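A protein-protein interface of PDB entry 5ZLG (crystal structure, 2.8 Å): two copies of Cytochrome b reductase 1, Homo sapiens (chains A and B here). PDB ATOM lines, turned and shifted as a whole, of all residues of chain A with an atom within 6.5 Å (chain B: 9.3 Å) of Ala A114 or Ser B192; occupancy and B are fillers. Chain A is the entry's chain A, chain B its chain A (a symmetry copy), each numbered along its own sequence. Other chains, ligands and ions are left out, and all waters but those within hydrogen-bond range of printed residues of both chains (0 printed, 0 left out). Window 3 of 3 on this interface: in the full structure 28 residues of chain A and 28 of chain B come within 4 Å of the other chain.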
ATOM      1  N   HIS A 108       0.535  13.539   3.058  1.00  0.00           N
ATOM      2  CA  HIS A 108       0.168  14.136   1.780  1.00  0.00           C
ATOM      3  C   HIS A 108      -1.289  13.884   1.439  1.00  0.00           C
ATOM      4  O   HIS A 108      -2.002  14.816   1.056  1.00  0.00           O
ATOM      5  CB  HIS A 108       1.079  13.619   0.674  1.00  0.00           C
ATOM      6  CG  HIS A 108       2.319  14.435   0.514  1.00  0.00           C
ATOM      7  ND1 HIS A 108       3.208  14.251  -0.522  1.00  0.00           N
ATOM      8  CD2 HIS A 108       2.814  15.448   1.265  1.00  0.00           C
ATOM      9  CE1 HIS A 108       4.201  15.114  -0.400  1.00  0.00           C
ATOM     10  NE2 HIS A 108       3.985  15.852   0.677  1.00  0.00           N
ATOM     11  N   ASN A 112      -3.868  16.904   1.107  1.00  0.00           N
ATOM     12  CA  ASN A 112      -4.145  17.153  -0.313  1.00  0.00           C
ATOM     13  C   ASN A 112      -2.933  17.756  -1.037  1.00  0.00           C
ATOM     14  O   ASN A 112      -2.967  18.872  -1.566  1.00  0.00           O
ATOM     15  CB  ASN A 112      -5.385  18.036  -0.478  1.00  0.00           C
ATOM     16  CG  ASN A 112      -6.584  17.263  -1.013  1.00  0.00           C
ATOM     17  OD1 ASN A 112      -7.616  17.151  -0.353  1.00  0.00           O
ATOM     18  ND2 ASN A 112      -6.446  16.724  -2.219  1.00  0.00           N
ATOM     19  N   ILE A 113      -1.846  16.988  -1.034  1.00  0.00           N
ATOM     20  CA  ILE A 113      -0.666  17.270  -1.837  1.00  0.00           C
ATOM     21  C   ILE A 113      -0.540  16.137  -2.854  1.00  0.00           C
ATOM     22  O   ILE A 113      -1.219  15.115  -2.764  1.00  0.00           O
ATOM     23  CB  ILE A 113       0.606  17.433  -0.960  1.00  0.00           C
ATOM     24  CG1 ILE A 113       0.421  18.593   0.025  1.00  0.00           C
ATOM     25  CG2 ILE A 113       1.874  17.693  -1.772  1.00  0.00           C
ATOM     26  CD1 ILE A 113       1.681  18.968   0.793  1.00  0.00           C
ATOM     27  N   ALA A 114       0.308  16.336  -3.850  1.00  0.00           N
ATOM     28  CA  ALA A 114       0.475  15.339  -4.892  1.00  0.00           C
ATOM     29  C   ALA A 114       1.576  14.351  -4.532  1.00  0.00           C
ATOM     30  O   ALA A 114       2.506  14.660  -3.781  1.00  0.00           O
ATOM     31  CB  ALA A 114       0.790  16.011  -6.231  1.00  0.00           C
ATOM     32  N   ASN A 115       1.472  13.155  -5.101  1.00  0.00           N
ATOM     33  CA  ASN A 115       2.412  12.074  -4.859  1.00  0.00           C
ATOM     34  C   ASN A 115       3.222  11.767  -6.108  1.00  0.00           C
ATOM     35  O   ASN A 115       2.696  11.783  -7.224  1.00  0.00           O
ATOM     36  CB  ASN A 115       1.678  10.809  -4.416  1.00  0.00           C
ATOM     37  CG  ASN A 115       1.052  10.948  -3.053  1.00  0.00           C
ATOM     38  OD1 ASN A 115       1.482  11.754  -2.222  1.00  0.00           O
ATOM     39  ND2 ASN A 115       0.031  10.150  -2.806  1.00  0.00           N
ATOM     40  N   MET A 116       4.505  11.476  -5.909  1.00  0.00           N
ATOM     41  CA  MET A 116       5.357  10.897  -6.943  1.00  0.00           C
ATOM     42  C   MET A 116       5.543  11.829  -8.131  1.00  0.00           C
ATOM     43  O   MET A 116       5.701  11.365  -9.262  1.00  0.00           O
ATOM     44  CB  MET A 116       4.813   9.553  -7.419  1.00  0.00           C
ATOM     45  CG  MET A 116       4.570   8.566  -6.288  1.00  0.00           C
ATOM     46  SD  MET A 116       6.034   8.388  -5.257  1.00  0.00           S
ATOM     47  CE  MET A 116       7.191   7.723  -6.449  1.00  0.00           C
ATOM     48  N   TYR A 117       5.525  13.142  -7.886  1.00  0.00           N
ATOM     49  CA  TYR A 117       5.788  14.120  -8.934  1.00  0.00           C
ATOM     50  C   TYR A 117       7.261  14.450  -9.071  1.00  0.00           C
ATOM     51  O   TYR A 117       7.664  15.022 -10.089  1.00  0.00           O
ATOM     52  CB  TYR A 117       5.013  15.423  -8.665  1.00  0.00           C
ATOM     53  CG  TYR A 117       5.507  16.201  -7.472  1.00  0.00           C
ATOM     54  CD1 TYR A 117       4.926  16.032  -6.225  1.00  0.00           C
ATOM     55  CD2 TYR A 117       6.557  17.103  -7.587  1.00  0.00           C
ATOM     56  CE1 TYR A 117       5.385  16.744  -5.111  1.00  0.00           C
ATOM     57  CE2 TYR A 117       7.023  17.816  -6.476  1.00  0.00           C
ATOM     58  CZ  TYR A 117       6.430  17.630  -5.245  1.00  0.00           C
ATOM     59  OH  TYR A 117       6.886  18.321  -4.150  1.00  0.00           O
ATOM     60  N   LEU B 182      14.231  22.256 -11.042  1.00  0.00           N
ATOM     61  CA  LEU B 182      12.806  22.012 -11.220  1.00  0.00           C
ATOM     62  C   LEU B 182      11.971  22.719 -10.155  1.00  0.00           C
ATOM     63  O   LEU B 182      10.913  23.281 -10.465  1.00  0.00           O
ATOM     64  CB  LEU B 182      12.537  20.514 -11.194  1.00  0.00           C
ATOM     65  CG  LEU B 182      13.369  19.761 -12.227  1.00  0.00           C
ATOM     66  CD1 LEU B 182      12.843  18.346 -12.370  1.00  0.00           C
ATOM     67  CD2 LEU B 182      13.337  20.510 -13.538  1.00  0.00           C
ATOM     68  N   ILE B 183      12.419  22.699  -8.895  1.00  0.00           N
ATOM     69  CA  ILE B 183      11.647  23.335  -7.831  1.00  0.00           C
ATOM     70  C   ILE B 183      11.658  24.850  -7.990  1.00  0.00           C
ATOM     71  O   ILE B 183      10.618  25.509  -7.874  1.00  0.00           O
ATOM     72  CB  ILE B 183      12.180  22.913  -6.454  1.00  0.00           C
ATOM     73  CG1 ILE B 183      11.901  21.433  -6.206  1.00  0.00           C
ATOM     74  CG2 ILE B 183      11.543  23.754  -5.354  1.00  0.00           C
ATOM     75  CD1 ILE B 183      12.320  20.991  -4.849  1.00  0.00           C
ATOM     76  N   LEU B 186       9.751  25.512 -11.952  1.00  0.00           N
ATOM     77  CA  LEU B 186       8.413  25.055 -12.312  1.00  0.00           C
ATOM     78  C   LEU B 186       7.410  25.511 -11.256  1.00  0.00           C
ATOM     79  O   LEU B 186       6.857  24.722 -10.490  1.00  0.00           O
ATOM     80  CB  LEU B 186       8.396  23.544 -12.476  1.00  0.00           C
ATOM     81  CG  LEU B 186       8.700  22.997 -13.872  1.00  0.00           C
ATOM     82  CD1 LEU B 186      10.048  23.504 -14.382  1.00  0.00           C
ATOM     83  CD2 LEU B 186       8.647  21.478 -13.831  1.00  0.00           C
ATOM     84  N   ARG B 187       7.170  26.824 -11.239  1.00  0.00           N
ATOM     85  CA  ARG B 187       6.261  27.419 -10.265  1.00  0.00           C
ATOM     86  C   ARG B 187       4.814  27.447 -10.748  1.00  0.00           C
ATOM     87  O   ARG B 187       3.900  27.176  -9.962  1.00  0.00           O
ATOM     88  CB  ARG B 187       6.732  28.829  -9.911  1.00  0.00           C
ATOM     89  CG  ARG B 187       8.174  28.867  -9.435  1.00  0.00           C
ATOM     90  CD  ARG B 187       8.626  30.275  -9.088  1.00  0.00           C
ATOM     91  NE  ARG B 187       8.030  30.759  -7.844  1.00  0.00           N
ATOM     92  CZ  ARG B 187       8.169  31.998  -7.377  1.00  0.00           C
ATOM     93  NH1 ARG B 187       8.887  32.891  -8.047  1.00  0.00           N
ATOM     94  NH2 ARG B 187       7.587  32.345  -6.238  1.00  0.00           N
ATOM     95  N   ASP B 188       4.578  27.752 -12.034  1.00  0.00           N
ATOM     96  CA  ASP B 188       3.209  27.845 -12.539  1.00  0.00           C
ATOM     97  C   ASP B 188       3.150  27.550 -14.037  1.00  0.00           C
ATOM     98  O   ASP B 188       3.361  28.456 -14.854  1.00  0.00           O
ATOM     99  CB  ASP B 188       2.630  29.232 -12.246  1.00  0.00           C
ATOM    100  CG  ASP B 188       1.145  29.330 -12.567  1.00  0.00           C
ATOM    101  OD1 ASP B 188       0.584  28.368 -13.141  1.00  0.00           O
ATOM    102  OD2 ASP B 188       0.534  30.374 -12.246  1.00  0.00           O
ATOM    103  N   PRO B 189       2.839  26.307 -14.452  1.00  0.00           N
ATOM    104  CA  PRO B 189       2.475  25.082 -13.724  1.00  0.00           C
ATOM    105  C   PRO B 189       3.502  24.658 -12.697  1.00  0.00           C
ATOM    106  O   PRO B 189       4.691  24.589 -13.007  1.00  0.00           O
ATOM    107  CB  PRO B 189       2.400  24.018 -14.825  1.00  0.00           C
ATOM    108  CG  PRO B 189       2.251  24.766 -16.081  1.00  0.00           C
ATOM    109  CD  PRO B 189       2.978  26.054 -15.893  1.00  0.00           C
ATOM    110  N   ALA B 190       3.044  24.382 -11.485  1.00  0.00           N
ATOM    111  CA  ALA B 190       3.955  23.931 -10.446  1.00  0.00           C
ATOM    112  C   ALA B 190       4.414  22.507 -10.728  1.00  0.00           C
ATOM    113  O   ALA B 190       3.659  21.689 -11.260  1.00  0.00           O
ATOM    114  CB  ALA B 190       3.284  24.009  -9.078  1.00  0.00           C
ATOM    115  N   TYR B 191       5.672  22.228 -10.395  1.00  0.00           N
ATOM    116  CA  TYR B 191       6.246  20.882 -10.395  1.00  0.00           C
ATOM    117  C   TYR B 191       5.238  19.841  -9.912  1.00  0.00           C
ATOM    118  O   TYR B 191       5.094  18.773 -10.513  1.00  0.00           O
ATOM    119  CB  TYR B 191       7.485  20.881  -9.496  1.00  0.00           C
ATOM    120  CG  TYR B 191       8.485  19.753  -9.655  1.00  0.00           C
ATOM    121  CD1 TYR B 191       8.500  18.925 -10.775  1.00  0.00           C
ATOM    122  CD2 TYR B 191       9.436  19.533  -8.671  1.00  0.00           C
ATOM    123  CE1 TYR B 191       9.446  17.902 -10.895  1.00  0.00           C
ATOM    124  CE2 TYR B 191      10.372  18.527  -8.784  1.00  0.00           C
ATOM    125  CZ  TYR B 191      10.380  17.712  -9.886  1.00  0.00           C
ATOM    126  OH  TYR B 191      11.332  16.707  -9.949  1.00  0.00           O
ATOM    127  N   SER B 192       4.517  20.166  -8.833  1.00  0.00           N
ATOM    128  CA  SER B 192       3.566  19.230  -8.237  1.00  0.00           C
ATOM    129  C   SER B 192       2.506  18.784  -9.229  1.00  0.00           C
ATOM    130  O   SER B 192       1.961  17.683  -9.097  1.00  0.00           O
ATOM    131  CB  SER B 192       2.909  19.879  -7.028  1.00  0.00           C
ATOM    132  OG  SER B 192       3.658  21.016  -6.608  1.00  0.00           O
ATOM    133  N   THR B 193       2.206  19.618 -10.225  1.00  0.00           N
ATOM    134  CA  THR B 193       1.159  19.342 -11.201  1.00  0.00           C
ATOM    135  C   THR B 193       1.631  18.466 -12.348  1.00  0.00           C
ATOM    136  O   THR B 193       0.961  18.439 -13.391  1.00  0.00           O
ATOM    137  CB  THR B 193       0.593  20.651 -11.752  1.00  0.00           C
ATOM    138  OG1 THR B 193       1.632  21.380 -12.426  1.00  0.00           O
ATOM    139  CG2 THR B 193       0.023  21.510 -10.618  1.00  0.00           C
ATOM    140  N   PHE B 194       2.753  17.758 -12.193  1.00  0.00           N
ATOM    141  CA  PHE B 194       3.246  16.832 -13.211  1.00  0.00           C
ATOM    142  C   PHE B 194       3.403  17.422 -14.616  1.00  0.00           C
ATOM    143  O   PHE B 194       3.081  16.736 -15.597  1.00  0.00           O
ATOM    144  CB  PHE B 194       2.305  15.633 -13.309  1.00  0.00           C
ATOM    145  CG  PHE B 194       2.505  14.612 -12.239  1.00  0.00           C
ATOM    146  CD1 PHE B 194       1.849  14.727 -11.017  1.00  0.00           C
ATOM    147  CD2 PHE B 194       3.344  13.519 -12.458  1.00  0.00           C
ATOM    148  CE1 PHE B 194       2.028  13.766 -10.024  1.00  0.00           C
ATOM    149  CE2 PHE B 194       3.532  12.563 -11.484  1.00  0.00           C
ATOM    150  CZ  PHE B 194       2.874  12.685 -10.260  1.00  0.00           C
ATOM    151  N   PRO B 195       3.918  18.638 -14.781  1.00  0.00           N
ATOM    152  CA  PRO B 195       3.965  19.234 -16.119  1.00  0.00           C
ATOM    153  C   PRO B 195       4.922  18.471 -17.026  1.00  0.00           C
ATOM    154  O   PRO B 195       5.699  17.632 -16.548  1.00  0.00           O
ATOM    155  CB  PRO B 195       4.453  20.666 -15.848  1.00  0.00           C
ATOM    156  CG  PRO B 195       5.262  20.558 -14.623  1.00  0.00           C
ATOM    157  CD  PRO B 195       4.609  19.485 -13.788  1.00  0.00           C
ATOM    158  N   GLY B 198       8.524  18.476 -16.032  1.00  0.00           N
ATOM    159  CA  GLY B 198       8.750  17.671 -14.840  1.00  0.00           C
ATOM    160  C   GLY B 198       9.021  16.212 -15.162  1.00  0.00           C
ATOM    161  O   GLY B 198       9.959  15.602 -14.625  1.00  0.00           O
ATOM    162  N   VAL B 199       8.207  15.627 -16.047  1.00  0.00           N
ATOM    163  CA  VAL B 199       8.414  14.229 -16.419  1.00  0.00           C
ATOM    164  C   VAL B 199       9.677  14.082 -17.254  1.00  0.00           C
ATOM    165  O   VAL B 199      10.434  13.112 -17.106  1.00  0.00           O
ATOM    166  CB  VAL B 199       7.191  13.685 -17.173  1.00  0.00           C
ATOM    167  CG1 VAL B 199       7.424  12.235 -17.553  1.00  0.00           C
ATOM    168  CG2 VAL B 199       5.933  13.839 -16.335  1.00  0.00           C
ATOM    169  N   ASN B 202      12.693  14.486 -14.882  1.00  0.00           N
ATOM    170  CA  ASN B 202      12.788  13.303 -14.020  1.00  0.00           C
ATOM    171  C   ASN B 202      13.361  12.116 -14.788  1.00  0.00           C
ATOM    172  O   ASN B 202      14.206  11.365 -14.272  1.00  0.00           O
ATOM    173  CB  ASN B 202      11.418  12.933 -13.456  1.00  0.00           C
ATOM    174  CG  ASN B 202      10.919  13.897 -12.404  1.00  0.00           C
ATOM    175  OD1 ASN B 202      11.476  14.981 -12.200  1.00  0.00           O
ATOM    176  ND2 ASN B 202       9.845  13.504 -11.732  1.00  0.00           N
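Among the printed residues, merely in contact across the chains: Ala A114 with Ser B192, Asn A115 with Phe B194, Met A116 with Phe B194, Tyr A117 with Tyr B191, Tyr A117 with Ser B192 and Tyr A117 with Phe B194.
A ring nitrogen (ND1) of His A108 lies within hydrogen-bond range of the backbone carbonyl oxygen (O) of Ala A114 (3.4 Å). OD1 of Asn A115 sits close to ND1 of His A108, 3.5 Å away. The backbone NH (N) of Tyr B191 lies within hydrogen-bond range of the backbone carbonyl oxygen (O) of Leu B186. OH of Tyr B191 sits at hydrogen-bond distance from OD1 of Asn B202, 2.8 Å away. The backbone carbonyl oxygen of Gly B198 sits close to the side-chain amide oxygen of Asn B202, at 2.9 Å.
Hydrophobic or aromatic side chains of chain B that line the printed part of chain A: Tyr B191 and Phe B194. Among the printed residues, no Asp or Glu carboxylate lies within 4 Å of a Lys or Arg side-chain nitrogen of the other chain.
No position is printed for both chains. Of the 7 pairs that touch across the chains among the printed residues, none has its exchanged pair printed and touching as well.
The backbone carbonyl oxygen (O) of Tyr A117 lies within hydrogen-bond range of the side-chain amide nitrogen (ND2) of Asn B202 (3.1 Å).
Of the printed residues of chain B, Ala A114 touches Ser B192 (3.5 Å). Ser B192 touches just these residues of chain A: Ala A114 and Tyr A117. Of chain B, only Phe B194 (3.2 Å) comes within 4 Å of Asn A115. Of the printed residues of chain A, Tyr B191 touches Tyr A117. Printed residues of chain A within 4 Å of Phe B194: Asn A115, Met A116 and Tyr A117. Printed residues of chain A within 4 Å of Asn B202: Tyr A117. Printed residues of chain B within 4 Å of Tyr A117: Tyr B191 (3.5 Å), Ser B192 (3.7 Å), Phe B194 (3.5 Å) and Asn B202 (3.1 Å). Ile B183 touches none of the printed residues of chain A. Ala B190 touches none of the printed residues of chain A. The nearest printed residue of chain A that does not touch Asn B202 is Met A116 (5.3 Å).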
